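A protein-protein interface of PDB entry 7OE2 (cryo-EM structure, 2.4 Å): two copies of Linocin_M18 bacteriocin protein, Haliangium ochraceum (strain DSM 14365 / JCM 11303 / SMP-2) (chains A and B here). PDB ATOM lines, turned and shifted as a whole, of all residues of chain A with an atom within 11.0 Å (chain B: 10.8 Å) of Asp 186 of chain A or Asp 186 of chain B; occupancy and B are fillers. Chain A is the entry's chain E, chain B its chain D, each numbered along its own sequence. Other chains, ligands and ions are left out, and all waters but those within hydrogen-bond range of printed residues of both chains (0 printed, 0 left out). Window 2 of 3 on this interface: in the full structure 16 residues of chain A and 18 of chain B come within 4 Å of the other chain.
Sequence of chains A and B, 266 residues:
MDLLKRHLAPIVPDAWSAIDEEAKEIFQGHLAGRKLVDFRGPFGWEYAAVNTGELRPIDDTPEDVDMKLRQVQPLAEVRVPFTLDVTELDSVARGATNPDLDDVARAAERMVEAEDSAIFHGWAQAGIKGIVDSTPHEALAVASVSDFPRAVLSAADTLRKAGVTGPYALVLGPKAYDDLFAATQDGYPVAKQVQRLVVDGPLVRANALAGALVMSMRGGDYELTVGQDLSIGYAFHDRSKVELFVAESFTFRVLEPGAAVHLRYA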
ATOM      1  N   VAL A 145      36.635  -1.498  16.631  1.00  0.00           N
ATOM      2  CA  VAL A 145      35.823  -0.320  16.902  1.00  0.00           C
ATOM      3  C   VAL A 145      34.629  -0.674  17.785  1.00  0.00           C
ATOM      4  O   VAL A 145      34.229   0.116  18.648  1.00  0.00           O
ATOM      5  CB  VAL A 145      35.410   0.339  15.570  1.00  0.00           C
ATOM      6  CG1 VAL A 145      34.512  -0.581  14.764  1.00  0.00           C
ATOM      7  CG2 VAL A 145      34.750   1.666  15.812  1.00  0.00           C
ATOM      8  N   SER A 146      34.068  -1.873  17.620  1.00  0.00           N
ATOM      9  CA  SER A 146      32.937  -2.302  18.432  1.00  0.00           C
ATOM     10  C   SER A 146      33.296  -2.498  19.899  1.00  0.00           C
ATOM     11  O   SER A 146      32.389  -2.613  20.727  1.00  0.00           O
ATOM     12  CB  SER A 146      32.347  -3.592  17.868  1.00  0.00           C
ATOM     13  OG  SER A 146      33.264  -4.663  17.980  1.00  0.00           O
ATOM     14  N   ALA A 182      31.829   5.629  11.324  1.00  0.00           N
ATOM     15  CA  ALA A 182      31.347   4.798  10.231  1.00  0.00           C
ATOM     16  C   ALA A 182      30.807   3.444  10.682  1.00  0.00           C
ATOM     17  O   ALA A 182      30.098   2.794   9.910  1.00  0.00           O
ATOM     18  CB  ALA A 182      32.460   4.569   9.204  1.00  0.00           C
ATOM     19  N   ALA A 183      31.100   3.016  11.905  1.00  0.00           N
ATOM     20  CA  ALA A 183      30.889   1.631  12.302  1.00  0.00           C
ATOM     21  C   ALA A 183      29.435   1.332  12.642  1.00  0.00           C
ATOM     22  O   ALA A 183      28.732   2.151  13.237  1.00  0.00           O
ATOM     23  CB  ALA A 183      31.766   1.290  13.500  1.00  0.00           C
ATOM     24  N   THR A 184      28.995   0.139  12.264  1.00  0.00           N
ATOM     25  CA  THR A 184      27.708  -0.396  12.678  1.00  0.00           C
ATOM     26  C   THR A 184      27.915  -1.796  13.229  1.00  0.00           C
ATOM     27  O   THR A 184      28.782  -2.537  12.763  1.00  0.00           O
ATOM     28  CB  THR A 184      26.686  -0.432  11.523  1.00  0.00           C
ATOM     29  OG1 THR A 184      27.303  -0.944  10.339  1.00  0.00           O
ATOM     30  CG2 THR A 184      26.147   0.947  11.245  1.00  0.00           C
ATOM     31  N   GLN A 185      27.132  -2.141  14.239  1.00  0.00           N
ATOM     32  CA  GLN A 185      27.085  -3.491  14.784  1.00  0.00           C
ATOM     33  C   GLN A 185      25.690  -4.028  14.511  1.00  0.00           C
ATOM     34  O   GLN A 185      24.724  -3.601  15.149  1.00  0.00           O
ATOM     35  CB  GLN A 185      27.412  -3.495  16.277  1.00  0.00           C
ATOM     36  CG  GLN A 185      27.667  -4.872  16.880  1.00  0.00           C
ATOM     37  CD  GLN A 185      29.020  -5.458  16.511  1.00  0.00           C
ATOM     38  OE1 GLN A 185      29.640  -5.068  15.523  1.00  0.00           O
ATOM     39  NE2 GLN A 185      29.485  -6.403  17.315  1.00  0.00           N
ATOM     40  N   ASP A 186      25.589  -4.945  13.547  1.00  0.00           N
ATOM     41  CA  ASP A 186      24.304  -5.445  13.056  1.00  0.00           C
ATOM     42  C   ASP A 186      23.391  -4.296  12.643  1.00  0.00           C
ATOM     43  O   ASP A 186      22.202  -4.272  12.953  1.00  0.00           O
ATOM     44  CB  ASP A 186      23.628  -6.341  14.090  1.00  0.00           C
ATOM     45  CG  ASP A 186      24.509  -7.481  14.524  1.00  0.00           C
ATOM     46  OD1 ASP A 186      24.724  -8.405  13.715  1.00  0.00           O
ATOM     47  OD2 ASP A 186      25.006  -7.456  15.665  1.00  0.00           O
ATOM     48  N   GLY A 187      23.969  -3.320  11.947  1.00  0.00           N
ATOM     49  CA  GLY A 187      23.255  -2.174  11.462  1.00  0.00           C
ATOM     50  C   GLY A 187      23.140  -1.025  12.441  1.00  0.00           C
ATOM     51  O   GLY A 187      23.014   0.122  12.014  1.00  0.00           O
ATOM     52  N   TYR A 188      23.168  -1.304  13.732  1.00  0.00           N
ATOM     53  CA  TYR A 188      23.049  -0.249  14.728  1.00  0.00           C
ATOM     54  C   TYR A 188      24.362   0.521  14.829  1.00  0.00           C
ATOM     55  O   TYR A 188      25.421  -0.091  14.962  1.00  0.00           O
ATOM     56  CB  TYR A 188      22.666  -0.829  16.085  1.00  0.00           C
ATOM     57  CG  TYR A 188      22.127   0.198  17.047  1.00  0.00           C
ATOM     58  CD1 TYR A 188      22.978   0.920  17.871  1.00  0.00           C
ATOM     59  CD2 TYR A 188      20.770   0.456  17.122  1.00  0.00           C
ATOM     60  CE1 TYR A 188      22.494   1.865  18.740  1.00  0.00           C
ATOM     61  CE2 TYR A 188      20.275   1.399  17.990  1.00  0.00           C
ATOM     62  CZ  TYR A 188      21.140   2.099  18.800  1.00  0.00           C
ATOM     63  OH  TYR A 188      20.649   3.040  19.667  1.00  0.00           O
ATOM     64  N   PRO A 189      24.333   1.850  14.760  1.00  0.00           N
ATOM     65  CA  PRO A 189      25.586   2.616  14.767  1.00  0.00           C
ATOM     66  C   PRO A 189      26.232   2.620  16.145  1.00  0.00           C
ATOM     67  O   PRO A 189      25.597   2.952  17.146  1.00  0.00           O
ATOM     68  CB  PRO A 189      25.150   4.025  14.343  1.00  0.00           C
ATOM     69  CG  PRO A 189      23.704   3.922  13.990  1.00  0.00           C
ATOM     70  CD  PRO A 189      23.157   2.725  14.674  1.00  0.00           C
ATOM     71  N   VAL A 190      27.515   2.263  16.180  1.00  0.00           N
ATOM     72  CA  VAL A 190      28.251   2.166  17.435  1.00  0.00           C
ATOM     73  C   VAL A 190      28.374   3.531  18.102  1.00  0.00           C
ATOM     74  O   VAL A 190      28.299   3.648  19.332  1.00  0.00           O
ATOM     75  CB  VAL A 190      29.629   1.529  17.179  1.00  0.00           C
ATOM     76  CG1 VAL A 190      30.375   1.316  18.478  1.00  0.00           C
ATOM     77  CG2 VAL A 190      29.464   0.220  16.424  1.00  0.00           C
ATOM     78  N   ALA A 191      28.558   4.581  17.301  1.00  0.00           N
ATOM     79  CA  ALA A 191      28.738   5.914  17.859  1.00  0.00           C
ATOM     80  C   ALA A 191      27.521   6.364  18.653  1.00  0.00           C
ATOM     81  O   ALA A 191      27.661   7.144  19.593  1.00  0.00           O
ATOM     82  CB  ALA A 191      29.060   6.912  16.747  1.00  0.00           C
ATOM     83  N   GLN A 193      25.576   4.392  20.656  1.00  0.00           N
ATOM     84  CA  GLN A 193      25.763   3.809  21.979  1.00  0.00           C
ATOM     85  C   GLN A 193      26.868   4.525  22.747  1.00  0.00           C
ATOM     86  O   GLN A 193      26.707   4.869  23.929  1.00  0.00           O
ATOM     87  CB  GLN A 193      26.075   2.320  21.832  1.00  0.00           C
ATOM     88  CG  GLN A 193      26.023   1.545  23.113  1.00  0.00           C
ATOM     89  CD  GLN A 193      26.459   0.114  22.944  1.00  0.00           C
ATOM     90  OE1 GLN A 193      26.903  -0.285  21.873  1.00  0.00           O
ATOM     91  NE2 GLN A 193      26.331  -0.670  23.999  1.00  0.00           N
ATOM     92  N   VAL B 145      25.916   1.239  -1.619  1.00  0.00           N
ATOM     93  CA  VAL B 145      25.240   2.294  -0.877  1.00  0.00           C
ATOM     94  C   VAL B 145      25.662   2.282   0.590  1.00  0.00           C
ATOM     95  O   VAL B 145      25.796   3.342   1.213  1.00  0.00           O
ATOM     96  CB  VAL B 145      23.715   2.158  -1.063  1.00  0.00           C
ATOM     97  CG1 VAL B 145      23.205   0.864  -0.459  1.00  0.00           C
ATOM     98  CG2 VAL B 145      22.998   3.346  -0.487  1.00  0.00           C
ATOM     99  N   SER B 146      25.918   1.101   1.154  1.00  0.00           N
ATOM    100  CA  SER B 146      26.346   0.998   2.543  1.00  0.00           C
ATOM    101  C   SER B 146      27.727   1.593   2.789  1.00  0.00           C
ATOM    102  O   SER B 146      28.095   1.794   3.948  1.00  0.00           O
ATOM    103  CB  SER B 146      26.325  -0.462   2.991  1.00  0.00           C
ATOM    104  OG  SER B 146      27.287  -1.223   2.287  1.00  0.00           O
ATOM    105  N   ALA B 182      16.422   4.217   0.131  1.00  0.00           N
ATOM    106  CA  ALA B 182      15.799   2.906   0.235  1.00  0.00           C
ATOM    107  C   ALA B 182      16.623   1.897   1.028  1.00  0.00           C
ATOM    108  O   ALA B 182      16.077   0.874   1.447  1.00  0.00           O
ATOM    109  CB  ALA B 182      15.524   2.334  -1.159  1.00  0.00           C
ATOM    110  N   ALA B 183      17.904   2.163   1.263  1.00  0.00           N
ATOM    111  CA  ALA B 183      18.825   1.139   1.735  1.00  0.00           C
ATOM    112  C   ALA B 183      18.696   0.878   3.230  1.00  0.00           C
ATOM    113  O   ALA B 183      18.493   1.795   4.027  1.00  0.00           O
ATOM    114  CB  ALA B 183      20.260   1.536   1.414  1.00  0.00           C
ATOM    115  N   THR B 184      18.829  -0.390   3.601  1.00  0.00           N
ATOM    116  CA  THR B 184      18.939  -0.798   4.992  1.00  0.00           C
ATOM    117  C   THR B 184      20.143  -1.711   5.141  1.00  0.00           C
ATOM    118  O   THR B 184      20.470  -2.477   4.234  1.00  0.00           O
ATOM    119  CB  THR B 184      17.671  -1.517   5.497  1.00  0.00           C
ATOM    120  OG1 THR B 184      17.227  -2.469   4.526  1.00  0.00           O
ATOM    121  CG2 THR B 184      16.566  -0.526   5.761  1.00  0.00           C
ATOM    122  N   GLN B 185      20.813  -1.604   6.277  1.00  0.00           N
ATOM    123  CA  GLN B 185      21.894  -2.506   6.652  1.00  0.00           C
ATOM    124  C   GLN B 185      21.426  -3.267   7.880  1.00  0.00           C
ATOM    125  O   GLN B 185      21.354  -2.698   8.973  1.00  0.00           O
ATOM    126  CB  GLN B 185      23.188  -1.736   6.918  1.00  0.00           C
ATOM    127  CG  GLN B 185      24.439  -2.598   7.039  1.00  0.00           C
ATOM    128  CD  GLN B 185      24.946  -3.128   5.707  1.00  0.00           C
ATOM    129  OE1 GLN B 185      24.210  -3.204   4.725  1.00  0.00           O
ATOM    130  NE2 GLN B 185      26.220  -3.493   5.672  1.00  0.00           N
ATOM    131  N   ASP B 186      21.089  -4.543   7.692  1.00  0.00           N
ATOM    132  CA  ASP B 186      20.474  -5.366   8.733  1.00  0.00           C
ATOM    133  C   ASP B 186      19.239  -4.685   9.310  1.00  0.00           C
ATOM    134  O   ASP B 186      19.025  -4.651  10.521  1.00  0.00           O
ATOM    135  CB  ASP B 186      21.477  -5.710   9.831  1.00  0.00           C
ATOM    136  CG  ASP B 186      22.712  -6.378   9.289  1.00  0.00           C
ATOM    137  OD1 ASP B 186      22.617  -7.547   8.870  1.00  0.00           O
ATOM    138  OD2 ASP B 186      23.778  -5.737   9.265  1.00  0.00           O
ATOM    139  N   GLY B 187      18.424  -4.117   8.425  1.00  0.00           N
ATOM    140  CA  GLY B 187      17.207  -3.451   8.792  1.00  0.00           C
ATOM    141  C   GLY B 187      17.361  -1.991   9.164  1.00  0.00           C
ATOM    142  O   GLY B 187      16.409  -1.226   9.013  1.00  0.00           O
ATOM    143  N   TYR B 188      18.520  -1.594   9.654  1.00  0.00           N
ATOM    144  CA  TYR B 188      18.733  -0.208  10.046  1.00  0.00           C
ATOM    145  C   TYR B 188      18.918   0.660   8.806  1.00  0.00           C
ATOM    146  O   TYR B 188      19.723   0.321   7.937  1.00  0.00           O
ATOM    147  CB  TYR B 188      19.941  -0.085  10.968  1.00  0.00           C
ATOM    148  CG  TYR B 188      19.982   1.210  11.735  1.00  0.00           C
ATOM    149  CD1 TYR B 188      20.587   2.340  11.199  1.00  0.00           C
ATOM    150  CD2 TYR B 188      19.406   1.311  12.989  1.00  0.00           C
ATOM    151  CE1 TYR B 188      20.618   3.526  11.888  1.00  0.00           C
ATOM    152  CE2 TYR B 188      19.434   2.494  13.688  1.00  0.00           C
ATOM    153  CZ  TYR B 188      20.042   3.598  13.134  1.00  0.00           C
ATOM    154  OH  TYR B 188      20.071   4.778  13.830  1.00  0.00           O
ATOM    155  N   PRO B 189      18.194   1.770   8.684  1.00  0.00           N
ATOM    156  CA  PRO B 189      18.286   2.580   7.461  1.00  0.00           C
ATOM    157  C   PRO B 189      19.606   3.337   7.392  1.00  0.00           C
ATOM    158  O   PRO B 189      19.986   4.041   8.325  1.00  0.00           O
ATOM    159  CB  PRO B 189      17.091   3.537   7.573  1.00  0.00           C
ATOM    160  CG  PRO B 189      16.326   3.105   8.779  1.00  0.00           C
ATOM    161  CD  PRO B 189      17.252   2.345   9.652  1.00  0.00           C
ATOM    162  N   VAL B 190      20.289   3.195   6.257  1.00  0.00           N
ATOM    163  CA  VAL B 190      21.596   3.816   6.065  1.00  0.00           C
ATOM    164  C   VAL B 190      21.485   5.335   6.080  1.00  0.00           C
ATOM    165  O   VAL B 190      22.362   6.033   6.606  1.00  0.00           O
ATOM    166  CB  VAL B 190      22.225   3.301   4.758  1.00  0.00           C
ATOM    167  CG1 VAL B 190      23.627   3.843   4.586  1.00  0.00           C
ATOM    168  CG2 VAL B 190      22.223   1.781   4.744  1.00  0.00           C
ATOM    169  N   ALA B 191      20.405   5.870   5.510  1.00  0.00           N
ATOM    170  CA  ALA B 191      20.246   7.315   5.434  1.00  0.00           C
ATOM    171  C   ALA B 191      20.190   7.952   6.814  1.00  0.00           C
ATOM    172  O   ALA B 191      20.591   9.103   6.972  1.00  0.00           O
ATOM    173  CB  ALA B 191      18.999   7.667   4.623  1.00  0.00           C
ATOM    174  N   GLN B 193      22.013   7.007   9.547  1.00  0.00           N
ATOM    175  CA  GLN B 193      23.409   7.177   9.932  1.00  0.00           C
ATOM    176  C   GLN B 193      24.067   8.302   9.141  1.00  0.00           C
ATOM    177  O   GLN B 193      24.763   9.161   9.706  1.00  0.00           O
ATOM    178  CB  GLN B 193      24.151   5.856   9.725  1.00  0.00           C
ATOM    179  CG  GLN B 193      25.520   5.811  10.332  1.00  0.00           C
ATOM    180  CD  GLN B 193      26.261   4.544   9.999  1.00  0.00           C
ATOM    181  OE1 GLN B 193      25.787   3.725   9.219  1.00  0.00           O
ATOM    182  NE2 GLN B 193      27.431   4.371  10.590  1.00  0.00           N
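NE2 of Gln 193 of chain B is in hydrogen-bond range of O of Ala 182 of chain A.
The backbone NH (N) of Val 190 of chain A is in hydrogen-bond range of the backbone carbonyl oxygen (O) of Ala 183 of chain A (3.2 Å).
Gln 193 of chain B touches Ala 183 of chain A (NE2 to O, 3.7 Å).
Thr 184 of chain A touches Gln 193 of chain B.
Asp 186 of chain B touches Asp 186 of chain A.
Gly 187 of chain A touches Gln 185 of chain B.
Gly 187 of chain A touches Asp 186 of chain B.
O of Gly 187 of chain A touches CG of Tyr 188 of chain B (3.2 Å).
Pro 189 of chain A touches Tyr 188 of chain B (CD to CZ, 3.6 Å).
Asp 186 of chain A touches just one residue of chain B: Asp 186.
Asp 186 of chain B touches just these residues of chain A: Asp 186 (3.5 Å) and Gly 187 (3.6 Å).
No residue of chain B comes within 4 Å of Gln 185 of chain A.
Gly 187 of chain A touches just these residues of chain B: Gln 185 (3.2 Å), Asp 186 (3.6 Å) and Tyr 188 (3.2 Å).
No residue of chain A comes within 4 Å of Thr 184 of chain B.
No residue of chain A comes within 4 Å of Gly 187 of chain B.
Printed residues of chain B within 4 Å of Ala 182 of chain A: Gln 193.
Of the printed residues of chain B, Ala 183 of chain A touches Gln 193 (3.7 Å).
Of the printed residues of chain A, Gln 193 of chain B touches Ala 182 (3.2 Å), Ala 183 (3.7 Å) and Thr 184 (3.5 Å).
Val 190 of chain A touches none of the printed residues of chain B.
The nearest residue of chain B that does not touch Asp 186 of chain A is Gln 185 of chain B (4.4 Å).
Hydrophobic or aromatic side chains of chain A that line the printed part of chain B: Pro 189.
Of the 13 printed residues of chain B, 4 touch a printed residue of chain A.
Printed residues of chain B that touch a printed residue of chain A: Gln 185, Asp 186, Tyr 188 and Gln 193.
Among the printed residues, no Asp or Glu carboxylate lies within 4 Å of a Lys or Arg side-chain nitrogen of the other chain.
Thr 184 of chain A touches Gln 193 of chain B, but with the chains exchanged Gln 193 of chain A does not touch Thr 184 of chain B (17.5 Å).
Gly 187 of chain A touches Asp 186 of chain B, but with the chains exchanged Asp 186 of chain A does not touch Gly 187 of chain B (5.9 Å).
Gly 187 of chain A touches Tyr 188 of chain B, but with the chains exchanged Tyr 188 of chain A does not touch Gly 187 of chain B (7.4 Å).
Pro 189 of chain A touches Tyr 188 of chain B, but with the chains exchanged Tyr 188 of chain A does not touch Pro 189 of chain B (7.7 Å).
Positions printed for both chains: 145, 146, 182, 183, 184, 185, 186, 187, 188, 189, 190, 191 and 193.
Of the 8 pairs that touch across the chains among the printed residues, 1 has its exchanged pair printed and touching as well.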
